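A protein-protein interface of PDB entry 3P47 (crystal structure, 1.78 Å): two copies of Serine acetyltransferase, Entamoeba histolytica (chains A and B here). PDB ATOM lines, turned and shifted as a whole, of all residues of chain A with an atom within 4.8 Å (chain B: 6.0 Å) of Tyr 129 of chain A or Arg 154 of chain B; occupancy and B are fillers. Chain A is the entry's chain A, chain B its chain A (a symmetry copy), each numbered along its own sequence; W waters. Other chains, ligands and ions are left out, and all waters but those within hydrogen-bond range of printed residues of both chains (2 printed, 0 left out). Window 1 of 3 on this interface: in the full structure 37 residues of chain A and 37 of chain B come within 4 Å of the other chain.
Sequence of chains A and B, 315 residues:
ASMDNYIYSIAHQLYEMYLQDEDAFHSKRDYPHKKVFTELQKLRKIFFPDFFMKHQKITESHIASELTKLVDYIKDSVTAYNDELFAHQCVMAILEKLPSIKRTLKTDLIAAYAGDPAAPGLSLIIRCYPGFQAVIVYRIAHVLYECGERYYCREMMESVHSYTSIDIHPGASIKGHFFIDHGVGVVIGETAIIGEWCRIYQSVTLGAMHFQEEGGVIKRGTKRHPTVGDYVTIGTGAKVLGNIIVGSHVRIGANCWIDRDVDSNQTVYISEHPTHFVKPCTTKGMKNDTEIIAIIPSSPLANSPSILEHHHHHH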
ATOM      1  N   ASP A 116      22.712 -17.832 -22.133  1.00  0.00           N
ATOM      2  CA  ASP A 116      21.648 -18.797 -22.463  1.00  0.00           C
ATOM      3  C   ASP A 116      20.394 -18.736 -21.569  1.00  0.00           C
ATOM      4  O   ASP A 116      20.392 -19.268 -20.456  1.00  0.00           O
ATOM      5  CB  ASP A 116      22.213 -20.233 -22.489  1.00  0.00           C
ATOM      6  CG  ASP A 116      21.156 -21.280 -22.915  1.00  0.00           C
ATOM      7  OD1 ASP A 116      20.093 -20.865 -23.427  1.00  0.00           O
ATOM      8  OD2 ASP A 116      21.398 -22.500 -22.751  1.00  0.00           O
ATOM      9  N   ALA A 118      17.872 -20.455 -21.587  1.00  0.00           N
ATOM     10  CA  ALA A 118      17.330 -21.764 -21.238  1.00  0.00           C
ATOM     11  C   ALA A 118      18.082 -22.459 -20.098  1.00  0.00           C
ATOM     12  O   ALA A 118      17.622 -23.473 -19.580  1.00  0.00           O
ATOM     13  CB  ALA A 118      17.229 -22.685 -22.515  1.00  0.00           C
ATOM     14  N   ALA A 119      19.212 -21.904 -19.643  1.00  0.00           N
ATOM     15  CA  ALA A 119      19.995 -22.550 -18.577  1.00  0.00           C
ATOM     16  C   ALA A 119      19.450 -22.205 -17.187  1.00  0.00           C
ATOM     17  O   ALA A 119      19.356 -21.036 -16.861  1.00  0.00           O
ATOM     18  CB  ALA A 119      21.460 -22.130 -18.646  1.00  0.00           C
ATOM     19  N   LEU A 124      23.498 -27.677 -14.589  1.00  0.00           N
ATOM     20  CA  LEU A 124      23.024 -28.379 -15.802  1.00  0.00           C
ATOM     21  C   LEU A 124      24.070 -28.228 -16.896  1.00  0.00           C
ATOM     22  O   LEU A 124      24.231 -29.111 -17.729  1.00  0.00           O
ATOM     23  CB  LEU A 124      21.683 -27.815 -16.282  1.00  0.00           C
ATOM     24  CG  LEU A 124      20.997 -28.638 -17.396  1.00  0.00           C
ATOM     25  CD1 LEU A 124      20.705 -29.983 -16.836  1.00  0.00           C
ATOM     26  CD2 LEU A 124      19.712 -27.959 -17.809  1.00  0.00           C
ATOM     27  N   ILE A 125      24.747 -27.079 -16.912  1.00  0.00           N
ATOM     28  CA  ILE A 125      25.735 -26.784 -17.925  1.00  0.00           C
ATOM     29  C   ILE A 125      26.918 -27.718 -17.723  1.00  0.00           C
ATOM     30  O   ILE A 125      27.351 -28.415 -18.634  1.00  0.00           O
ATOM     31  CB  ILE A 125      26.173 -25.296 -17.891  1.00  0.00           C
ATOM     32  CG1 ILE A 125      24.964 -24.364 -18.082  1.00  0.00           C
ATOM     33  CG2 ILE A 125      27.226 -25.067 -19.005  1.00  0.00           C
ATOM     34  CD1 ILE A 125      25.286 -22.851 -17.923  1.00  0.00           C
ATOM     35  N   ARG A 127      26.855 -30.611 -16.114  1.00  0.00           N
ATOM     36  CA  ARG A 127      26.442 -32.015 -16.284  1.00  0.00           C
ATOM     37  C   ARG A 127      26.254 -32.415 -17.742  1.00  0.00           C
ATOM     38  O   ARG A 127      26.500 -33.569 -18.056  1.00  0.00           O
ATOM     39  CB  ARG A 127      25.076 -32.284 -15.581  1.00  0.00           C
ATOM     40  CG  ARG A 127      25.143 -32.304 -14.066  1.00  0.00           C
ATOM     41  CD  ARG A 127      25.659 -33.590 -13.579  1.00  0.00           C
ATOM     42  NE  ARG A 127      24.815 -34.679 -14.070  1.00  0.00           N
ATOM     43  CZ  ARG A 127      25.129 -35.963 -14.011  1.00  0.00           C
ATOM     44  NH1 ARG A 127      26.284 -36.384 -13.460  1.00  0.00           N
ATOM     45  NH2 ARG A 127      24.275 -36.841 -14.525  1.00  0.00           N
ATOM     46  N   CYS A 128      25.726 -31.523 -18.600  1.00  0.00           N
ATOM     47  CA  CYS A 128      25.324 -31.979 -19.950  1.00  0.00           C
ATOM     48  C   CYS A 128      25.414 -30.979 -21.145  1.00  0.00           C
ATOM     49  O   CYS A 128      25.106 -31.370 -22.286  1.00  0.00           O
ATOM     50  CB  CYS A 128      23.905 -32.605 -19.871  1.00  0.00           C
ATOM     51  SG  CYS A 128      22.600 -31.366 -19.752  1.00  0.00           S
ATOM     52  N   TYR A 129      25.833 -29.728 -20.938  1.00  0.00           N
ATOM     53  CA  TYR A 129      25.909 -28.808 -22.088  1.00  0.00           C
ATOM     54  C   TYR A 129      27.068 -29.290 -22.956  1.00  0.00           C
ATOM     55  O   TYR A 129      28.156 -29.444 -22.444  1.00  0.00           O
ATOM     56  CB  TYR A 129      26.139 -27.344 -21.676  1.00  0.00           C
ATOM     57  CG  TYR A 129      24.811 -26.590 -21.495  1.00  0.00           C
ATOM     58  CD1 TYR A 129      24.669 -25.289 -21.991  1.00  0.00           C
ATOM     59  CD2 TYR A 129      23.712 -27.201 -20.855  1.00  0.00           C
ATOM     60  CE1 TYR A 129      23.452 -24.589 -21.849  1.00  0.00           C
ATOM     61  CE2 TYR A 129      22.509 -26.520 -20.678  1.00  0.00           C
ATOM     62  CZ  TYR A 129      22.385 -25.216 -21.187  1.00  0.00           C
ATOM     63  OH  TYR A 129      21.197 -24.537 -21.087  1.00  0.00           O
ATOM     64  N   PRO A 130      26.814 -29.530 -24.260  1.00  0.00           N
ATOM     65  CA  PRO A 130      27.830 -30.133 -25.149  1.00  0.00           C
ATOM     66  C   PRO A 130      28.940 -29.149 -25.479  1.00  0.00           C
ATOM     67  O   PRO A 130      30.098 -29.544 -25.551  1.00  0.00           O
ATOM     68  CB  PRO A 130      27.019 -30.508 -26.413  1.00  0.00           C
ATOM     69  CG  PRO A 130      25.845 -29.554 -26.402  1.00  0.00           C
ATOM     70  CD  PRO A 130      25.492 -29.457 -24.911  1.00  0.00           C
ATOM     71  N   GLY A 131      28.594 -27.867 -25.664  1.00  0.00           N
ATOM     72  CA  GLY A 131      29.636 -26.845 -25.845  1.00  0.00           C
ATOM     73  C   GLY A 131      30.638 -26.892 -24.689  1.00  0.00           C
ATOM     74  O   GLY A 131      31.862 -26.703 -24.897  1.00  0.00           O
ATOM     75  N   PHE A 132      30.131 -27.092 -23.479  1.00  0.00           N
ATOM     76  CA  PHE A 132      31.025 -27.104 -22.291  1.00  0.00           C
ATOM     77  C   PHE A 132      31.838 -28.398 -22.230  1.00  0.00           C
ATOM     78  O   PHE A 132      33.044 -28.382 -21.910  1.00  0.00           O
ATOM     79  CB  PHE A 132      30.250 -26.857 -20.981  1.00  0.00           C
ATOM     80  CG  PHE A 132      31.149 -26.694 -19.781  1.00  0.00           C
ATOM     81  CD1 PHE A 132      31.989 -25.583 -19.692  1.00  0.00           C
ATOM     82  CD2 PHE A 132      31.209 -27.665 -18.793  1.00  0.00           C
ATOM     83  CE1 PHE A 132      32.856 -25.446 -18.593  1.00  0.00           C
ATOM     84  CE2 PHE A 132      32.059 -27.499 -17.692  1.00  0.00           C
ATOM     85  CZ  PHE A 132      32.892 -26.390 -17.614  1.00  0.00           C
ATOM     86  N   GLN A 133      31.208 -29.531 -22.544  1.00  0.00           N
ATOM     87  CA  GLN A 133      31.985 -30.786 -22.603  1.00  0.00           C
ATOM     88  C   GLN A 133      33.129 -30.659 -23.584  1.00  0.00           C
ATOM     89  O   GLN A 133      34.243 -31.088 -23.275  1.00  0.00           O
ATOM     90  CB  GLN A 133      31.114 -31.985 -22.991  1.00  0.00           C
ATOM     91  CG  GLN A 133      29.793 -32.082 -22.196  1.00  0.00           C
ATOM     92  CD  GLN A 133      29.976 -32.026 -20.681  1.00  0.00           C
ATOM     93  OE1 GLN A 133      30.711 -32.831 -20.124  1.00  0.00           O
ATOM     94  NE2 GLN A 133      29.276 -31.080 -20.005  1.00  0.00           N
ATOM     95  N   PHE A 179      31.709 -19.588 -25.041  1.00  0.00           N
ATOM     96  CA  PHE A 179      30.451 -20.328 -25.063  1.00  0.00           C
ATOM     97  C   PHE A 179      30.071 -20.696 -26.488  1.00  0.00           C
ATOM     98  O   PHE A 179      29.941 -19.821 -27.336  1.00  0.00           O
ATOM     99  CB  PHE A 179      29.344 -19.496 -24.399  1.00  0.00           C
ATOM    100  CG  PHE A 179      27.950 -20.147 -24.403  1.00  0.00           C
ATOM    101  CD1 PHE A 179      27.787 -21.479 -24.077  1.00  0.00           C
ATOM    102  CD2 PHE A 179      26.820 -19.357 -24.614  1.00  0.00           C
ATOM    103  CE1 PHE A 179      26.494 -22.069 -24.039  1.00  0.00           C
ATOM    104  CE2 PHE A 179      25.514 -19.919 -24.553  1.00  0.00           C
ATOM    105  CZ  PHE A 179      25.381 -21.274 -24.269  1.00  0.00           C
ATOM    106  N   ALA B 141      10.303 -36.750 -22.755  1.00  0.00           N
ATOM    107  CA  ALA B 141      10.926 -35.542 -22.136  1.00  0.00           C
ATOM    108  C   ALA B 141      10.018 -34.307 -22.008  1.00  0.00           C
ATOM    109  O   ALA B 141      10.128 -33.522 -21.042  1.00  0.00           O
ATOM    110  CB  ALA B 141      12.215 -35.159 -22.902  1.00  0.00           C
ATOM    111  N   GLU B 149       9.636 -29.861 -14.654  1.00  0.00           N
ATOM    112  CA  GLU B 149      11.005 -30.360 -14.434  1.00  0.00           C
ATOM    113  C   GLU B 149      11.918 -29.666 -15.439  1.00  0.00           C
ATOM    114  O   GLU B 149      11.482 -29.363 -16.563  1.00  0.00           O
ATOM    115  CB  GLU B 149      11.048 -31.908 -14.502  1.00  0.00           C
ATOM    116  CG  GLU B 149      12.168 -32.559 -13.692  1.00  0.00           C
ATOM    117  CD  GLU B 149      13.519 -32.554 -14.433  1.00  0.00           C
ATOM    118  OE1 GLU B 149      13.515 -32.694 -15.670  1.00  0.00           O
ATOM    119  OE2 GLU B 149      14.576 -32.441 -13.789  1.00  0.00           O
ATOM    120  N   ARG B 150      13.146 -29.313 -15.022  1.00  0.00           N
ATOM    121  CA  ARG B 150      13.972 -28.477 -15.873  1.00  0.00           C
ATOM    122  C   ARG B 150      15.387 -28.990 -16.076  1.00  0.00           C
ATOM    123  O   ARG B 150      16.158 -28.378 -16.830  1.00  0.00           O
ATOM    124  CB  ARG B 150      14.026 -27.030 -15.318  1.00  0.00           C
ATOM    125  CG  ARG B 150      12.676 -26.314 -15.340  1.00  0.00           C
ATOM    126  CD  ARG B 150      12.309 -25.976 -16.749  1.00  0.00           C
ATOM    127  NE  ARG B 150      11.033 -25.276 -16.894  1.00  0.00           N
ATOM    128  CZ  ARG B 150       9.840 -25.880 -16.952  1.00  0.00           C
ATOM    129  NH1 ARG B 150       9.719 -27.207 -16.841  1.00  0.00           N
ATOM    130  NH2 ARG B 150       8.755 -25.148 -17.137  1.00  0.00           N
ATOM    131  N   TYR B 151      15.730 -30.069 -15.402  1.00  0.00           N
ATOM    132  CA  TYR B 151      17.108 -30.586 -15.421  1.00  0.00           C
ATOM    133  C   TYR B 151      17.229 -31.929 -16.134  1.00  0.00           C
ATOM    134  O   TYR B 151      17.893 -32.017 -17.177  1.00  0.00           O
ATOM    135  CB  TYR B 151      17.694 -30.712 -14.010  1.00  0.00           C
ATOM    136  CG  TYR B 151      18.072 -29.370 -13.435  1.00  0.00           C
ATOM    137  CD1 TYR B 151      19.407 -28.935 -13.401  1.00  0.00           C
ATOM    138  CD2 TYR B 151      17.080 -28.509 -12.958  1.00  0.00           C
ATOM    139  CE1 TYR B 151      19.739 -27.676 -12.883  1.00  0.00           C
ATOM    140  CE2 TYR B 151      17.386 -27.246 -12.468  1.00  0.00           C
ATOM    141  CZ  TYR B 151      18.706 -26.836 -12.411  1.00  0.00           C
ATOM    142  OH  TYR B 151      18.974 -25.574 -11.920  1.00  0.00           O
ATOM    143  N   TYR B 152      16.671 -32.990 -15.544  1.00  0.00           N
ATOM    144  CA  TYR B 152      16.798 -34.316 -16.183  1.00  0.00           C
ATOM    145  C   TYR B 152      16.210 -34.374 -17.608  1.00  0.00           C
ATOM    146  O   TYR B 152      16.790 -35.029 -18.503  1.00  0.00           O
ATOM    147  CB  TYR B 152      16.302 -35.472 -15.266  1.00  0.00           C
ATOM    148  CG  TYR B 152      16.183 -36.805 -15.982  1.00  0.00           C
ATOM    149  CD1 TYR B 152      17.310 -37.479 -16.453  1.00  0.00           C
ATOM    150  CD2 TYR B 152      14.926 -37.373 -16.208  1.00  0.00           C
ATOM    151  CE1 TYR B 152      17.183 -38.667 -17.150  1.00  0.00           C
ATOM    152  CE2 TYR B 152      14.789 -38.584 -16.885  1.00  0.00           C
ATOM    153  CZ  TYR B 152      15.909 -39.213 -17.363  1.00  0.00           C
ATOM    154  OH  TYR B 152      15.775 -40.405 -18.063  1.00  0.00           O
ATOM    155  N   CYS B 153      15.090 -33.691 -17.844  1.00  0.00           N
ATOM    156  CA  CYS B 153      14.502 -33.701 -19.196  1.00  0.00           C
ATOM    157  C   CYS B 153      15.475 -33.113 -20.222  1.00  0.00           C
ATOM    158  O   CYS B 153      15.556 -33.570 -21.352  1.00  0.00           O
ATOM    159  CB  CYS B 153      13.121 -33.024 -19.227  1.00  0.00           C
ATOM    160  SG  CYS B 153      13.091 -31.224 -18.822  1.00  0.00           S
ATOM    161  N   ARG B 154      16.257 -32.117 -19.824  1.00  0.00           N
ATOM    162  CA  ARG B 154      17.298 -31.630 -20.727  1.00  0.00           C
ATOM    163  C   ARG B 154      18.441 -32.641 -20.899  1.00  0.00           C
ATOM    164  O   ARG B 154      18.956 -32.795 -22.027  1.00  0.00           O
ATOM    165  CB  ARG B 154      17.822 -30.268 -20.227  1.00  0.00           C
ATOM    166  CG  ARG B 154      18.973 -29.685 -21.065  1.00  0.00           C
ATOM    167  CD  ARG B 154      18.570 -29.293 -22.492  1.00  0.00           C
ATOM    168  NE  ARG B 154      19.729 -28.773 -23.253  1.00  0.00           N
ATOM    169  CZ  ARG B 154      20.142 -27.502 -23.230  1.00  0.00           C
ATOM    170  NH1 ARG B 154      19.514 -26.584 -22.486  1.00  0.00           N
ATOM    171  NH2 ARG B 154      21.195 -27.149 -23.949  1.00  0.00           N
ATOM    172  N   GLU B 155      18.848 -33.308 -19.818  1.00  0.00           N
ATOM    173  CA  GLU B 155      19.880 -34.337 -19.924  1.00  0.00           C
ATOM    174  C   GLU B 155      19.411 -35.458 -20.844  1.00  0.00           C
ATOM    175  O   GLU B 155      20.195 -35.957 -21.667  1.00  0.00           O
ATOM    176  CB  GLU B 155      20.241 -34.908 -18.557  1.00  0.00           C
ATOM    177  CG  GLU B 155      21.423 -35.867 -18.556  1.00  0.00           C
ATOM    178  CD  GLU B 155      21.955 -36.059 -17.121  1.00  0.00           C
ATOM    179  OE1 GLU B 155      21.169 -36.329 -16.209  1.00  0.00           O
ATOM    180  OE2 GLU B 155      23.156 -35.891 -16.905  1.00  0.00           O
ATOM    181  N   MET B 156      18.136 -35.852 -20.731  1.00  0.00           N
ATOM    182  CA  MET B 156      17.609 -36.901 -21.648  1.00  0.00           C
ATOM    183  C   MET B 156      17.757 -36.488 -23.120  1.00  0.00           C
ATOM    184  O   MET B 156      18.184 -37.294 -23.994  1.00  0.00           O
ATOM    185  CB  MET B 156      16.122 -37.163 -21.340  1.00  0.00           C
ATOM    186  CG  MET B 156      15.556 -38.434 -21.983  1.00  0.00           C
ATOM    187  SD  MET B 156      13.756 -38.595 -21.666  1.00  0.00           S
ATOM    188  CE  MET B 156      13.728 -37.841 -20.101  1.00  0.00           C
ATOM    189  N   MET B 157      17.412 -35.234 -23.410  1.00  0.00           N
ATOM    190  CA  MET B 157      17.480 -34.726 -24.777  1.00  0.00           C
ATOM    191  C   MET B 157      18.932 -34.502 -25.240  1.00  0.00           C
ATOM    192  O   MET B 157      19.225 -34.511 -26.446  1.00  0.00           O
ATOM    193  CB  MET B 157      16.648 -33.467 -24.952  1.00  0.00           C
ATOM    194  CG  MET B 157      15.144 -33.670 -24.712  1.00  0.00           C
ATOM    195  SD  MET B 157      14.532 -35.144 -25.621  1.00  0.00           S
ATOM    196  CE  MET B 157      14.684 -34.618 -27.326  1.00  0.00           C
ATOM    197  N   GLU B 158      19.836 -34.265 -24.282  1.00  0.00           N
ATOM    198  CA  GLU B 158      21.259 -34.249 -24.640  1.00  0.00           C
ATOM    199  C   GLU B 158      21.796 -35.635 -25.063  1.00  0.00           C
ATOM    200  O   GLU B 158      22.736 -35.729 -25.879  1.00  0.00           O
ATOM    201  CB  GLU B 158      22.119 -33.625 -23.518  1.00  0.00           C
ATOM    202  CG  GLU B 158      21.974 -32.079 -23.448  1.00  0.00           C
ATOM    203  CD  GLU B 158      22.208 -31.351 -24.736  1.00  0.00           C
ATOM    204  OE1 GLU B 158      23.038 -31.780 -25.558  1.00  0.00           O
ATOM    205  OE2 GLU B 158      21.582 -30.297 -24.916  1.00  0.00           O
ATOM    206  N   SER B 159      21.246 -36.708 -24.498  1.00  0.00           N
ATOM    207  CA  SER B 159      21.515 -38.032 -25.048  1.00  0.00           C
ATOM    208  C   SER B 159      21.068 -38.148 -26.517  1.00  0.00           C
ATOM    209  O   SER B 159      21.797 -38.695 -27.339  1.00  0.00           O
ATOM    210  CB  SER B 159      20.893 -39.150 -24.192  1.00  0.00           C
ATOM    211  OG  SER B 159      21.591 -39.222 -22.947  1.00  0.00           O
ATOM    212  N   ASP B 167      18.780 -31.494 -31.903  1.00  0.00           N
ATOM    213  CA  ASP B 167      18.821 -30.734 -30.660  1.00  0.00           C
ATOM    214  C   ASP B 167      17.437 -30.184 -30.425  1.00  0.00           C
ATOM    215  O   ASP B 167      17.119 -29.103 -30.917  1.00  0.00           O
ATOM    216  CB  ASP B 167      19.801 -29.580 -30.872  1.00  0.00           C
ATOM    217  CG  ASP B 167      20.203 -28.845 -29.589  1.00  0.00           C
ATOM    218  OD1 ASP B 167      19.602 -29.025 -28.499  1.00  0.00           O
ATOM    219  OD2 ASP B 167      21.180 -28.039 -29.719  1.00  0.00           O
ATOM    220  N   ILE B 168      16.619 -30.927 -29.673  1.00  0.00           N
ATOM    221  CA  ILE B 168      15.264 -30.473 -29.354  1.00  0.00           C
ATOM    222  C   ILE B 168      15.138 -30.221 -27.869  1.00  0.00           C
ATOM    223  O   ILE B 168      15.365 -31.119 -27.068  1.00  0.00           O
ATOM    224  CB  ILE B 168      14.199 -31.497 -29.810  1.00  0.00           C
ATOM    225  CG1 ILE B 168      14.337 -31.776 -31.295  1.00  0.00           C
ATOM    226  CG2 ILE B 168      12.798 -31.002 -29.531  1.00  0.00           C
ATOM    227  CD1 ILE B 168      13.401 -32.984 -31.741  1.00  0.00           C
ATOM    228  N   HIS B 169      14.844 -28.974 -27.487  1.00  0.00           N
ATOM    229  CA  HIS B 169      14.646 -28.665 -26.064  1.00  0.00           C
ATOM    230  C   HIS B 169      13.359 -29.326 -25.596  1.00  0.00           C
ATOM    231  O   HIS B 169      12.375 -29.309 -26.334  1.00  0.00           O
ATOM    232  CB  HIS B 169      14.587 -27.143 -25.841  1.00  0.00           C
ATOM    233  CG  HIS B 169      14.669 -26.767 -24.403  1.00  0.00           C
ATOM    234  ND1 HIS B 169      15.857 -26.403 -23.789  1.00  0.00           N
ATOM    235  CD2 HIS B 169      13.737 -26.829 -23.429  1.00  0.00           C
ATOM    236  CE1 HIS B 169      15.619 -26.194 -22.500  1.00  0.00           C
ATOM    237  NE2 HIS B 169      14.352 -26.470 -22.257  1.00  0.00           N
ATOM    238  N   PRO B 170      13.368 -29.936 -24.396  1.00  0.00           N
ATOM    239  CA  PRO B 170      12.184 -30.639 -23.913  1.00  0.00           C
ATOM    240  C   PRO B 170      10.948 -29.750 -23.760  1.00  0.00           C
ATOM    241  O   PRO B 170       9.845 -30.253 -23.805  1.00  0.00           O
ATOM    242  CB  PRO B 170      12.630 -31.212 -22.543  1.00  0.00           C
ATOM    243  CG  PRO B 170      13.872 -30.448 -22.141  1.00  0.00           C
ATOM    244  CD  PRO B 170      14.521 -30.120 -23.490  1.00  0.00           C
HETATM  245  O   HOH W   1      20.998 -24.123 -24.796  1.00  0.00           O
HETATM  246  O   HOH W   2      17.556 -26.151 -20.376  1.00  0.00           O
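NH2 of Arg 127 of chain A lies within salt-bridge range of OE2 of Glu 155 of chain B. The side-chain hydroxyl (OH) of Tyr 129 of chain A lies within hydrogen-bond range of the guanidinium group (NH1) of Arg 154 of chain B (3.0 Å).
The side-chain carboxylate (OD1) of Asp 116 of chain A is in hydrogen-bond range of the backbone NH (N) of Ala 118 of chain A. OD2 of Asp 116 of chain A is in hydrogen-bond range of OH of Tyr 129 of chain A (2.6 Å). The backbone carbonyl oxygen (O) of Leu 124 of chain A is in hydrogen-bond range of the side-chain sulfur (SG) of Cys 128 of chain A (3.4 Å). The backbone carbonyl oxygen of Tyr 129 of chain A sits close to the side-chain amide nitrogen of Gln 133 of chain A. The side-chain carboxylate (OE2) of Glu 149 of chain B lies within hydrogen-bond range of the backbone NH (N) of Tyr 151 of chain B (3.1 Å). OE2 of Glu 158 of chain B is in salt-bridge range of NE of Arg 154 of chain B, at 2.9 Å.
Among the printed residues, pairs that only touch across the chains: Cys 128 of chain A with Glu 158 of chain B (3.4 Å), Pro 130 of chain A with Glu 158 of chain B (3.4 Å), Leu 124 of chain A with Tyr 151 of chain B (3.5 Å), Leu 124 of chain A with Arg 150 of chain B (3.7 Å), Leu 124 of chain A with Arg 154 of chain B (3.8 Å) and Ala 118 of chain A with His 169 of chain B (3.9 Å).
Printed residues of chain B within 4 Å of Leu 124 of chain A: Arg 150, Tyr 151 and Arg 154. Printed residues of chain B within 4 Å of Arg 127 of chain A: Glu 155 (2.8 Å). Of the printed residues of chain B, Cys 128 of chain A touches Glu 158. Tyr 129 of chain A touches just one residue of chain B: Arg 154. Ala 141 of chain B touches none of the printed residues of chain A. Of chain A, only Leu 124 (3.8 Å) and Tyr 129 (3.0 Å) come within 4 Å of Arg 154 of chain B. Printed residues of chain A within 4 Å of Glu 155 of chain B: Arg 127 (2.8 Å). Of the printed residues of chain A, Glu 158 of chain B touches Cys 128 (3.4 Å) and Pro 130 (3.4 Å). Pro 170 of chain B touches none of the printed residues of chain A.
Hydrophobic or aromatic side chains of chain B that line the printed part of chain A: Tyr 151 and His 169. Among the printed residues, Asp or Glu carboxylates within 4 Å of a Lys or Arg side-chain nitrogen of the other chain: Arg 127 of chain A with Glu 155 of chain B (2.8 Å).
No position is printed for both chains. Of the 8 pairs that touch across the chains among the printed residues, none has its exchanged pair printed and touching as well.
Water W1 bridges OD2 of Asp 116 of chain A (2.6 Å) and NH2 of Arg 154 of chain B (3.1 Å). Water W2 lies within hydrogen-bond range of the backbone carbonyl oxygen of Ala 118 of chain A (2.8 Å) and the guanidinium group of Arg 154 of chain B (2.9 Å).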
